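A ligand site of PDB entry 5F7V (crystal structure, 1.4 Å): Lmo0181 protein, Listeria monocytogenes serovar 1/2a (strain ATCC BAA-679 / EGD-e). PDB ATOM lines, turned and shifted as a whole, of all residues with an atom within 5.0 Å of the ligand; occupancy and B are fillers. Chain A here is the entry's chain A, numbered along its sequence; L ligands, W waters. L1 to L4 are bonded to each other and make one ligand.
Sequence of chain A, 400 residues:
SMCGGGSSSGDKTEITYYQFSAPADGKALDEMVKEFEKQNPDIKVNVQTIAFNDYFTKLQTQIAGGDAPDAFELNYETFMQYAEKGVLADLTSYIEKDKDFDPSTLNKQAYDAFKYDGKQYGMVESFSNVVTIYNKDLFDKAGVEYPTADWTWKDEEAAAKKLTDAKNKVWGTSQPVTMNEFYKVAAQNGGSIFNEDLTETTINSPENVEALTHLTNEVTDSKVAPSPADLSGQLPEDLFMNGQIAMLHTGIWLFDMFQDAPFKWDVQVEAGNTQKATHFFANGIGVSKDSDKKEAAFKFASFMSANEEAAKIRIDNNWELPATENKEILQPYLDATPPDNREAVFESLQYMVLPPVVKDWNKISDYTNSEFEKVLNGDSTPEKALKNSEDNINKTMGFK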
ATOM      1  N   PHE A  20     -13.970  -7.166 -23.169  1.00  0.00           N
ATOM      2  CA  PHE A  20     -14.947  -7.371 -22.112  1.00  0.00           C
ATOM      3  C   PHE A  20     -15.446  -8.776 -21.937  1.00  0.00           C
ATOM      4  O   PHE A  20     -15.873  -9.105 -20.859  1.00  0.00           O
ATOM      5  CB  PHE A  20     -16.190  -6.466 -22.270  1.00  0.00           C
ATOM      6  CG  PHE A  20     -16.939  -6.738 -23.547  1.00  0.00           C
ATOM      7  CD1 PHE A  20     -17.895  -7.744 -23.639  1.00  0.00           C
ATOM      8  CD2 PHE A  20     -16.644  -6.002 -24.671  1.00  0.00           C
ATOM      9  CE1 PHE A  20     -18.486  -8.008 -24.871  1.00  0.00           C
ATOM     10  CE2 PHE A  20     -17.266  -6.225 -25.863  1.00  0.00           C
ATOM     11  CZ  PHE A  20     -18.196  -7.249 -25.976  1.00  0.00           C
ATOM     12  N   SER A  21     -15.445  -9.613 -22.980  1.00  0.00           N
ATOM     13  CA  SER A  21     -16.261 -10.827 -22.874  1.00  0.00           C
ATOM     14  C   SER A  21     -15.646 -11.972 -22.080  1.00  0.00           C
ATOM     15  O   SER A  21     -16.390 -12.824 -21.630  1.00  0.00           O
ATOM     16  CB  SER A  21     -16.669 -11.303 -24.264  1.00  0.00           C
ATOM     17  OG  SER A  21     -15.594 -11.858 -25.010  1.00  0.00           O
ATOM     18  N   PHE A  52     -18.270  -5.252 -18.648  1.00  0.00           N
ATOM     19  CA  PHE A  52     -19.192  -4.932 -19.741  1.00  0.00           C
ATOM     20  C   PHE A  52     -19.957  -3.648 -19.495  1.00  0.00           C
ATOM     21  O   PHE A  52     -20.173  -2.883 -20.422  1.00  0.00           O
ATOM     22  CB  PHE A  52     -20.169  -6.103 -19.977  1.00  0.00           C
ATOM     23  CG  PHE A  52     -21.125  -5.895 -21.117  1.00  0.00           C
ATOM     24  CD1 PHE A  52     -20.698  -6.020 -22.436  1.00  0.00           C
ATOM     25  CD2 PHE A  52     -22.459  -5.595 -20.879  1.00  0.00           C
ATOM     26  CE1 PHE A  52     -21.603  -5.859 -23.456  1.00  0.00           C
ATOM     27  CE2 PHE A  52     -23.363  -5.425 -21.910  1.00  0.00           C
ATOM     28  CZ  PHE A  52     -22.923  -5.549 -23.200  1.00  0.00           C
ATOM     29  N   ASN A  75     -19.314  -5.462 -29.696  1.00  0.00           N
ATOM     30  CA  ASN A  75     -20.498  -6.293 -29.852  1.00  0.00           C
ATOM     31  C   ASN A  75     -21.271  -5.873 -31.100  1.00  0.00           C
ATOM     32  O   ASN A  75     -21.052  -4.822 -31.690  1.00  0.00           O
ATOM     33  CB  ASN A  75     -21.336  -6.342 -28.550  1.00  0.00           C
ATOM     34  CG  ASN A  75     -21.897  -5.015 -28.135  1.00  0.00           C
ATOM     35  OD1 ASN A  75     -21.647  -4.012 -28.744  1.00  0.00           O
ATOM     36  ND2 ASN A  75     -22.626  -5.056 -27.045  1.00  0.00           N
ATOM     37  N   GLU A  77     -24.279  -4.874 -31.365  1.00  0.00           N
ATOM     38  CA  GLU A  77     -25.150  -3.704 -31.300  1.00  0.00           C
ATOM     39  C   GLU A  77     -24.389  -2.401 -31.147  1.00  0.00           C
ATOM     40  O   GLU A  77     -25.011  -1.374 -31.345  1.00  0.00           O
ATOM     41  CB  GLU A  77     -26.260  -3.908 -30.261  1.00  0.00           C
ATOM     42  CG  GLU A  77     -25.814  -4.179 -28.835  1.00  0.00           C
ATOM     43  CD  GLU A  77     -25.524  -5.641 -28.476  1.00  0.00           C
ATOM     44  OE1 GLU A  77     -24.940  -6.394 -29.299  1.00  0.00           O
ATOM     45  OE2 GLU A  77     -25.850  -6.054 -27.339  1.00  0.00           O
ATOM     46  N   SER A 128     -23.484 -15.849 -29.689  1.00  0.00           N
ATOM     47  CA  SER A 128     -24.207 -16.339 -28.498  1.00  0.00           C
ATOM     48  C   SER A 128     -25.692 -16.015 -28.571  1.00  0.00           C
ATOM     49  O   SER A 128     -26.147 -15.295 -29.452  1.00  0.00           O
ATOM     50  CB  SER A 128     -23.609 -15.657 -27.255  1.00  0.00           C
ATOM     51  OG  SER A 128     -23.832 -14.259 -27.251  1.00  0.00           O
ATOM     52  N   VAL A 130     -29.564 -16.291 -25.866  1.00  0.00           N
ATOM     53  CA  VAL A 130     -30.171 -16.317 -24.537  1.00  0.00           C
ATOM     54  C   VAL A 130     -31.133 -17.478 -24.472  1.00  0.00           C
ATOM     55  O   VAL A 130     -31.749 -17.865 -25.458  1.00  0.00           O
ATOM     56  CB  VAL A 130     -30.874 -14.980 -24.271  1.00  0.00           C
ATOM     57  CG1 VAL A 130     -31.819 -15.021 -23.060  1.00  0.00           C
ATOM     58  CG2 VAL A 130     -29.820 -13.861 -24.108  1.00  0.00           C
ATOM     59  N   PRO A 176     -34.521  -9.524 -17.845  1.00  0.00           N
ATOM     60  CA  PRO A 176     -34.269  -8.065 -17.921  1.00  0.00           C
ATOM     61  C   PRO A 176     -35.435  -7.318 -18.567  1.00  0.00           C
ATOM     62  O   PRO A 176     -36.093  -7.801 -19.480  1.00  0.00           O
ATOM     63  CB  PRO A 176     -33.007  -7.992 -18.791  1.00  0.00           C
ATOM     64  CG  PRO A 176     -32.352  -9.333 -18.609  1.00  0.00           C
ATOM     65  CD  PRO A 176     -33.472 -10.294 -18.548  1.00  0.00           C
ATOM     66  N   THR A 178     -35.253  -4.245 -20.357  1.00  0.00           N
ATOM     67  CA  THR A 178     -34.290  -3.357 -20.972  1.00  0.00           C
ATOM     68  C   THR A 178     -34.574  -3.284 -22.465  1.00  0.00           C
ATOM     69  O   THR A 178     -35.290  -4.126 -23.007  1.00  0.00           O
ATOM     70  CB  THR A 178     -32.852  -3.875 -20.786  1.00  0.00           C
ATOM     71  OG1 THR A 178     -32.782  -5.147 -21.483  1.00  0.00           O
ATOM     72  CG2 THR A 178     -32.464  -3.980 -19.330  1.00  0.00           C
ATOM     73  N   ASN A 180     -32.461  -3.983 -24.755  1.00  0.00           N
ATOM     74  CA  ASN A 180     -31.882  -5.167 -25.417  1.00  0.00           C
ATOM     75  C   ASN A 180     -32.785  -6.362 -25.284  1.00  0.00           C
ATOM     76  O   ASN A 180     -32.957  -7.120 -26.248  1.00  0.00           O
ATOM     77  CB  ASN A 180     -30.504  -5.509 -24.838  1.00  0.00           C
ATOM     78  CG  ASN A 180     -29.402  -5.414 -25.857  1.00  0.00           C
ATOM     79  OD1 ASN A 180     -29.373  -4.511 -26.709  1.00  0.00           O
ATOM     80  ND2 ASN A 180     -28.479  -6.363 -25.775  1.00  0.00           N
ATOM     81  N   GLU A 181     -33.426  -6.503 -24.133  1.00  0.00           N
ATOM     82  CA  GLU A 181     -34.348  -7.643 -23.983  1.00  0.00           C
ATOM     83  C   GLU A 181     -35.619  -7.395 -24.795  1.00  0.00           C
ATOM     84  O   GLU A 181     -36.245  -8.304 -25.339  1.00  0.00           O
ATOM     85  CB  GLU A 181     -34.682  -7.845 -22.522  1.00  0.00           C
ATOM     86  CG  GLU A 181     -35.317  -9.204 -22.237  1.00  0.00           C
ATOM     87  CD  GLU A 181     -34.343 -10.372 -22.302  1.00  0.00           C
ATOM     88  OE1 GLU A 181     -33.098 -10.196 -22.434  1.00  0.00           O
ATOM     89  OE2 GLU A 181     -34.861 -11.515 -22.189  1.00  0.00           O
ATOM     90  N   LEU A 235     -26.844  -8.759  -8.867  1.00  0.00           N
ATOM     91  CA  LEU A 235     -27.301  -9.078 -10.207  1.00  0.00           C
ATOM     92  C   LEU A 235     -28.173 -10.306 -10.135  1.00  0.00           C
ATOM     93  O   LEU A 235     -28.051 -11.128  -9.224  1.00  0.00           O
ATOM     94  CB  LEU A 235     -26.098  -9.307 -11.125  1.00  0.00           C
ATOM     95  CG  LEU A 235     -25.256  -8.054 -11.399  1.00  0.00           C
ATOM     96  CD1 LEU A 235     -23.991  -8.459 -12.145  1.00  0.00           C
ATOM     97  CD2 LEU A 235     -26.007  -6.950 -12.136  1.00  0.00           C
ATOM     98  N   PRO A 236     -29.085 -10.485 -11.103  1.00  0.00           N
ATOM     99  CA  PRO A 236     -29.948 -11.646 -11.057  1.00  0.00           C
ATOM    100  C   PRO A 236     -29.231 -12.990 -10.991  1.00  0.00           C
ATOM    101  O   PRO A 236     -29.666 -13.923 -10.311  1.00  0.00           O
ATOM    102  CB  PRO A 236     -30.842 -11.510 -12.287  1.00  0.00           C
ATOM    103  CG  PRO A 236     -30.640 -10.149 -12.784  1.00  0.00           C
ATOM    104  CD  PRO A 236     -29.397  -9.559 -12.207  1.00  0.00           C
ATOM    105  N   GLU A 237     -28.116 -13.120 -11.708  1.00  0.00           N
ATOM    106  CA  GLU A 237     -27.364 -14.370 -11.664  1.00  0.00           C
ATOM    107  C   GLU A 237     -26.843 -14.677 -10.252  1.00  0.00           C
ATOM    108  O   GLU A 237     -26.692 -15.838  -9.888  1.00  0.00           O
ATOM    109  CB  GLU A 237     -26.225 -14.352 -12.679  1.00  0.00           C
ATOM    110  CG  GLU A 237     -25.283 -13.218 -12.558  1.00  0.00           C
ATOM    111  CD  GLU A 237     -25.656 -12.000 -13.421  1.00  0.00           C
ATOM    112  OE1 GLU A 237     -26.842 -11.699 -13.792  1.00  0.00           O
ATOM    113  OE2 GLU A 237     -24.668 -11.303 -13.778  1.00  0.00           O
ATOM    114  N   HIS A 249     -33.756 -15.758 -17.417  1.00  0.00           N
ATOM    115  CA  HIS A 249     -33.550 -15.532 -18.868  1.00  0.00           C
ATOM    116  C   HIS A 249     -32.228 -14.804 -19.058  1.00  0.00           C
ATOM    117  O   HIS A 249     -32.109 -13.617 -18.744  1.00  0.00           O
ATOM    118  CB  HIS A 249     -34.710 -14.674 -19.424  1.00  0.00           C
ATOM    119  CG  HIS A 249     -36.018 -15.387 -19.358  1.00  0.00           C
ATOM    120  ND1 HIS A 249     -36.632 -15.879 -20.476  1.00  0.00           N
ATOM    121  CD2 HIS A 249     -36.813 -15.707 -18.317  1.00  0.00           C
ATOM    122  CE1 HIS A 249     -37.755 -16.473 -20.136  1.00  0.00           C
ATOM    123  NE2 HIS A 249     -37.883 -16.380 -18.821  1.00  0.00           N
ATOM    124  N   THR A 250     -31.237 -15.548 -19.516  1.00  0.00           N
ATOM    125  CA  THR A 250     -29.896 -14.977 -19.612  1.00  0.00           C
ATOM    126  C   THR A 250     -29.082 -15.729 -20.627  1.00  0.00           C
ATOM    127  O   THR A 250     -29.522 -16.716 -21.222  1.00  0.00           O
ATOM    128  CB  THR A 250     -29.220 -14.925 -18.227  1.00  0.00           C
ATOM    129  OG1 THR A 250     -28.120 -14.021 -18.281  1.00  0.00           O
ATOM    130  CG2 THR A 250     -28.793 -16.288 -17.769  1.00  0.00           C
ATOM    131  N   GLY A 251     -27.893 -15.208 -20.866  1.00  0.00           N
ATOM    132  CA  GLY A 251     -27.090 -15.771 -21.948  1.00  0.00           C
ATOM    133  C   GLY A 251     -26.278 -16.981 -21.621  1.00  0.00           C
ATOM    134  O   GLY A 251     -25.930 -17.286 -20.476  1.00  0.00           O
ATOM    135  N   TRP A 253     -23.317 -17.161 -22.072  1.00  0.00           N
ATOM    136  CA  TRP A 253     -22.075 -16.649 -21.457  1.00  0.00           C
ATOM    137  C   TRP A 253     -22.025 -16.833 -19.963  1.00  0.00           C
ATOM    138  O   TRP A 253     -20.971 -16.609 -19.385  1.00  0.00           O
ATOM    139  CB  TRP A 253     -21.821 -15.170 -21.818  1.00  0.00           C
ATOM    140  CG  TRP A 253     -22.960 -14.268 -21.552  1.00  0.00           C
ATOM    141  CD1 TRP A 253     -23.225 -13.577 -20.401  1.00  0.00           C
ATOM    142  CD2 TRP A 253     -23.997 -13.920 -22.476  1.00  0.00           C
ATOM    143  NE1 TRP A 253     -24.379 -12.867 -20.530  1.00  0.00           N
ATOM    144  CE2 TRP A 253     -24.863 -13.032 -21.801  1.00  0.00           C
ATOM    145  CE3 TRP A 253     -24.280 -14.240 -23.822  1.00  0.00           C
ATOM    146  CZ2 TRP A 253     -26.004 -12.490 -22.420  1.00  0.00           C
ATOM    147  CZ3 TRP A 253     -25.395 -13.680 -24.415  1.00  0.00           C
ATOM    148  CH2 TRP A 253     -26.259 -12.832 -23.737  1.00  0.00           C
ATOM    149  N   LEU A 254     -23.132 -17.235 -19.339  1.00  0.00           N
ATOM    150  CA  LEU A 254     -23.110 -17.544 -17.901  1.00  0.00           C
ATOM    151  C   LEU A 254     -23.026 -19.038 -17.611  1.00  0.00           C
ATOM    152  O   LEU A 254     -23.026 -19.413 -16.447  1.00  0.00           O
ATOM    153  CB  LEU A 254     -24.320 -16.937 -17.178  1.00  0.00           C
ATOM    154  CG  LEU A 254     -24.241 -15.407 -17.154  1.00  0.00           C
ATOM    155  CD1 LEU A 254     -25.435 -14.856 -16.357  1.00  0.00           C
ATOM    156  CD2 LEU A 254     -22.931 -14.816 -16.644  1.00  0.00           C
ATOM    157  N   HIS A 279     -32.698 -14.207 -29.063  1.00  0.00           N
ATOM    158  CA  HIS A 279     -31.540 -13.310 -29.273  1.00  0.00           C
ATOM    159  C   HIS A 279     -30.475 -13.994 -30.106  1.00  0.00           C
ATOM    160  O   HIS A 279     -30.274 -15.190 -30.076  1.00  0.00           O
ATOM    161  CB  HIS A 279     -30.940 -12.933 -27.931  1.00  0.00           C
ATOM    162  CG  HIS A 279     -31.570 -11.727 -27.327  1.00  0.00           C
ATOM    163  ND1 HIS A 279     -31.958 -11.669 -26.005  1.00  0.00           N
ATOM    164  CD2 HIS A 279     -31.811 -10.494 -27.841  1.00  0.00           C
ATOM    165  CE1 HIS A 279     -32.419 -10.457 -25.740  1.00  0.00           C
ATOM    166  NE2 HIS A 279     -32.329  -9.733 -26.834  1.00  0.00           N
ATOM    167  N   PHE A 281     -26.419 -12.722 -30.650  1.00  0.00           N
ATOM    168  CA  PHE A 281     -25.361 -11.752 -30.343  1.00  0.00           C
ATOM    169  C   PHE A 281     -24.069 -12.238 -30.953  1.00  0.00           C
ATOM    170  O   PHE A 281     -23.862 -13.410 -31.168  1.00  0.00           O
ATOM    171  CB  PHE A 281     -25.256 -11.586 -28.825  1.00  0.00           C
ATOM    172  CG  PHE A 281     -26.455 -10.932 -28.208  1.00  0.00           C
ATOM    173  CD1 PHE A 281     -26.829  -9.643 -28.604  1.00  0.00           C
ATOM    174  CD2 PHE A 281     -27.144 -11.550 -27.200  1.00  0.00           C
ATOM    175  CE1 PHE A 281     -27.932  -9.052 -28.041  1.00  0.00           C
ATOM    176  CE2 PHE A 281     -28.255 -10.947 -26.638  1.00  0.00           C
ATOM    177  CZ  PHE A 281     -28.636  -9.689 -27.050  1.00  0.00           C
ATOM    178  N   ALA A 282     -23.164 -11.311 -31.203  1.00  0.00           N
ATOM    179  CA  ALA A 282     -21.835 -11.647 -31.689  1.00  0.00           C
ATOM    180  C   ALA A 282     -20.823 -10.645 -31.260  1.00  0.00           C
ATOM    181  O   ALA A 282     -21.132  -9.453 -31.219  1.00  0.00           O
ATOM    182  CB  ALA A 282     -21.796 -11.746 -33.206  1.00  0.00           C
ATOM    183  N   ASN A 283     -19.627 -11.103 -30.916  1.00  0.00           N
ATOM    184  CA  ASN A 283     -18.505 -10.209 -30.648  1.00  0.00           C
ATOM    185  C   ASN A 283     -17.485 -10.303 -31.753  1.00  0.00           C
ATOM    186  O   ASN A 283     -17.286 -11.378 -32.308  1.00  0.00           O
ATOM    187  CB  ASN A 283     -17.875 -10.606 -29.329  1.00  0.00           C
ATOM    188  CG  ASN A 283     -18.867 -10.432 -28.184  1.00  0.00           C
ATOM    189  OD1 ASN A 283     -19.519  -9.409 -28.095  1.00  0.00           O
ATOM    190  ND2 ASN A 283     -18.960 -11.421 -27.288  1.00  0.00           N
ATOM    191  N   GLU A 320     -19.164 -18.897 -24.800  1.00  0.00           N
ATOM    192  CA  GLU A 320     -20.027 -18.616 -25.966  1.00  0.00           C
ATOM    193  C   GLU A 320     -19.754 -19.696 -27.012  1.00  0.00           C
ATOM    194  O   GLU A 320     -19.465 -20.830 -26.643  1.00  0.00           O
ATOM    195  CB  GLU A 320     -19.886 -17.195 -26.472  1.00  0.00           C
ATOM    196  CG  GLU A 320     -20.207 -16.182 -25.365  1.00  0.00           C
ATOM    197  CD  GLU A 320     -20.338 -14.759 -25.826  1.00  0.00           C
ATOM    198  OE1 GLU A 320     -20.091 -14.464 -27.045  1.00  0.00           O
ATOM    199  OE2 GLU A 320     -20.661 -13.943 -24.932  1.00  0.00           O
HETATM  200  C1  LIG L   1     -27.042  -7.643 -22.706  1.00  0.00           C
HETATM  201  C2  LIG L   1     -27.017  -7.749 -21.186  1.00  0.00           C
HETATM  202  C3  LIG L   1     -27.313  -9.195 -20.784  1.00  0.00           C
HETATM  203  C4  LIG L   1     -28.648  -9.616 -21.368  1.00  0.00           C
HETATM  204  C5  LIG L   1     -28.719  -9.317 -22.881  1.00  0.00           C
HETATM  205  C6  LIG L   1     -30.120  -9.483 -23.472  1.00  0.00           C
HETATM  206  O1  LIG L   1     -25.755  -7.311 -20.658  1.00  0.00           O
HETATM  207  O2  LIG L   1     -27.359  -9.206 -19.347  1.00  0.00           O
HETATM  208  O3  LIG L   1     -28.837 -11.037 -21.220  1.00  0.00           O
HETATM  209  O4  LIG L   1     -28.328  -7.992 -23.210  1.00  0.00           O
HETATM  210  O5  LIG L   1     -31.020  -8.610 -22.802  1.00  0.00           O
HETATM  211  C1  LG2 L   2     -27.171 -10.491 -18.743  1.00  0.00           C
HETATM  212  C2  LG2 L   2     -27.777 -10.368 -17.356  1.00  0.00           C
HETATM  213  C3  LG2 L   2     -26.956  -9.495 -16.444  1.00  0.00           C
HETATM  214  C4  LG2 L   2     -25.482  -9.899 -16.473  1.00  0.00           C
HETATM  215  C5  LG2 L   2     -24.976  -9.937 -17.898  1.00  0.00           C
HETATM  216  C6  LG2 L   2     -23.590 -10.556 -17.880  1.00  0.00           C
HETATM  217  O1  LG2 L   2     -29.132  -9.892 -17.425  1.00  0.00           O
HETATM  218  O2  LG2 L   2     -27.441  -9.410 -15.125  1.00  0.00           O
HETATM  219  O3  LG2 L   2     -24.711  -9.037 -15.656  1.00  0.00           O
HETATM  220  O4  LG2 L   2     -25.772 -10.840 -18.670  1.00  0.00           O
HETATM  221  O5  LG2 L   2     -22.990 -10.638 -19.179  1.00  0.00           O
HETATM  222  C1  LG3 L   3     -22.939 -10.775 -24.062  1.00  0.00           C
HETATM  223  C2  LG3 L   3     -22.384 -10.951 -25.459  1.00  0.00           C
HETATM  224  C3  LG3 L   3     -22.432  -9.624 -26.201  1.00  0.00           C
HETATM  225  C4  LG3 L   3     -23.836  -9.023 -26.136  1.00  0.00           C
HETATM  226  C5  LG3 L   3     -24.271  -8.883 -24.686  1.00  0.00           C
HETATM  227  C6  LG3 L   3     -25.711  -8.401 -24.546  1.00  0.00           C
HETATM  228  O1  LG3 L   3     -21.039 -11.441 -25.358  1.00  0.00           O
HETATM  229  O2  LG3 L   3     -22.095  -9.890 -27.560  1.00  0.00           O
HETATM  230  O3  LG3 L   3     -23.770  -7.707 -26.696  1.00  0.00           O
HETATM  231  O4  LG3 L   3     -24.236 -10.179 -24.057  1.00  0.00           O
HETATM  232  O5  LG3 L   3     -25.991  -8.516 -23.128  1.00  0.00           O
HETATM  233  C1  LG4 L   4     -22.371  -9.423 -19.600  1.00  0.00           C
HETATM  234  C2  LG4 L   4     -22.649  -9.269 -21.080  1.00  0.00           C
HETATM  235  C3  LG4 L   4     -21.947 -10.319 -21.917  1.00  0.00           C
HETATM  236  C4  LG4 L   4     -20.465 -10.260 -21.607  1.00  0.00           C
HETATM  237  C5  LG4 L   4     -20.279 -10.539 -20.106  1.00  0.00           C
HETATM  238  C6  LG4 L   4     -18.817 -10.577 -19.694  1.00  0.00           C
HETATM  239  O1  LG4 L   4     -24.061  -9.319 -21.287  1.00  0.00           O
HETATM  240  O2  LG4 L   4     -22.053  -9.990 -23.299  1.00  0.00           O
HETATM  241  O3  LG4 L   4     -19.727 -11.181 -22.418  1.00  0.00           O
HETATM  242  O4  LG4 L   4     -20.964  -9.514 -19.379  1.00  0.00           O
HETATM  243  O5  LG4 L   4     -18.304  -9.246 -19.772  1.00  0.00           O
HETATM  244  O   HOH W   1     -23.716  -6.805 -16.537  1.00  0.00           O
HETATM  245  O   HOH W   2     -28.791  -7.169 -14.428  1.00  0.00           O
HETATM  246  O   HOH W   3     -31.407 -11.842 -21.029  1.00  0.00           O
HETATM  247  O   HOH W   4     -25.217  -5.759 -18.551  1.00  0.00           O
HETATM  248  O   HOH W   5     -28.428 -13.311 -15.605  1.00  0.00           O
HETATM  249  O   HOH W   6     -23.619  -8.803 -29.706  1.00  0.00           O
HETATM  250  O   HOH W   7     -30.503  -6.581 -21.039  1.00  0.00           O
HETATM  251  O   HOH W   8     -21.829 -12.806 -28.417  1.00  0.00           O
HETATM  252  O   HOH W   9     -18.668 -14.118 -22.843  1.00  0.00           O
HETATM  253  O   HOH W  10     -18.576  -7.830 -17.396  1.00  0.00           O
HETATM  254  O   HOH W  11     -21.120  -8.175 -16.492  1.00  0.00           O
HETATM  255  O   HOH W  12     -29.631  -7.284 -18.474  1.00  0.00           O
HETATM  256  O   HOH W  13     -30.781 -11.971 -16.658  1.00  0.00           O
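Water W3 lies within hydrogen-bond range of an oxygen (O3) of LIG L1, the side-chain carboxylate (OE1) of Glu 181 and the backbone carbonyl oxygen (O) of His 249. Water W7 bridges the side-chain hydroxyl of Thr 178 (2.7 Å) and an oxygen (O5) of LIG L1 (2.7 Å). Water W13 lies within hydrogen-bond range of O1 of LG2 L2 (2.8 Å) and O of His 249 (3.0 Å). Water W10 bridges O5 of LG4 L4 and N of Phe 52. Water W8 lies within hydrogen-bond range of the side-chain hydroxyl (OG) of Ser 128 (2.7 Å), the side-chain carboxylate (OE1) of Glu 320 (2.8 Å), an oxygen (O2) of LG3 L3 (3.1 Å), the side-chain amide nitrogen (ND2) of Asn 283 (3.4 Å), the backbone NH (N) of Ala 282 (3.4 Å) and the backbone carbonyl oxygen (O) of Phe 281 (3.5 Å). Water W9 lies within hydrogen-bond range of the backbone carbonyl oxygen of Ser 21 (2.9 Å), the side-chain carboxylate of Glu 320 (2.9 Å) and an oxygen (O3) of LG4 L4 (3.2 Å).
Ser 21 touches the ligand. CE2 of Phe 52 touches O1 of LIG L1, 3.3 Å away. CG of Pro 176 touches O1 of LG2 L2 (3.5 Å). Leu 235 touches the ligand. CD of Pro 236 touches O2 of LG2 L2 (3.5 Å). OG1 of Thr 250 touches C1 of LG2 L2 (3.7 Å). His 279 touches the ligand. CB of Phe 281 touches O2 of LG3 L3 (3.8 Å). Ala 282 touches the ligand. Hydrophobic or aromatic side chains that line the ligand: Phe 52, Pro 176, Leu 235, Pro 236, Trp 253, His 279 and Phe 281. 18 residues have an atom within 4 Å of the ligand: Phe 20, Ser 21, Phe 52, Asn 75, Glu 77, Pro 176, Asn 180, Glu 181, Leu 235, Pro 236, Glu 237, Thr 250, Trp 253, His 279, Phe 281, Ala 282, Asn 283 and Glu 320. The nearest printed residue that does not touch the ligand is Ser 128 (4.03 Å).
The side-chain amide oxygen (OD1) of Asn 283 is in hydrogen-bond range of an oxygen (O2) of LG3 L3. OE2 of Glu 320 lies within hydrogen-bond range of O1 of LG3 L3 (2.6 Å). O of Phe 20 sits at hydrogen-bond distance from O5 of LG4 L4. The side-chain carboxylate (OE1) of Glu 181 lies within hydrogen-bond range of an oxygen (O5) of LIG L1, at 2.6 Å. The side-chain carboxylate (OE2) of Glu 77 lies within hydrogen-bond range of an oxygen (O3) of LG3 L3 (2.7 Å). ND2 of Asn 180 sits at hydrogen-bond distance from O4 of LIG L1 (3.0 Å). An oxygen (O5) of LG2 L2 sits at hydrogen-bond distance from the indole nitrogen (NE1) of Trp 253, at 3.0 Å. The side-chain carboxylate (OE1) of Glu 237 lies within hydrogen-bond range of an oxygen (O2) of LG2 L2. An oxygen (O3) of LG3 L3 lies within hydrogen-bond range of the side-chain amide nitrogen of Asn 75. N of Glu 181 is in hydrogen-bond range of O5 of LIG L1 (3.5 Å).
The backbone carbonyl oxygen (O) of Asn 180 lies within hydrogen-bond range of a ring nitrogen (NE2) of His 279, 2.8 Å away. OG1 of Thr 178 sits close to N of Asn 180, at 3.5 Å. ND2 of Asn 75 sits close to OE2 of Glu 77, at 3.4 Å. The backbone NH (N) of Phe 281 lies within hydrogen-bond range of the backbone carbonyl oxygen (O) of Ser 128 (2.9 Å). N of Glu 181 lies within hydrogen-bond range of OG1 of Thr 178 (3.0 Å). The side-chain amide nitrogen of Asn 180 sits at hydrogen-bond distance from the side-chain carboxylate of Glu 77. The side-chain carboxylate (OE1) of Glu 320 sits at hydrogen-bond distance from the side-chain amide nitrogen (ND2) of Asn 283.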
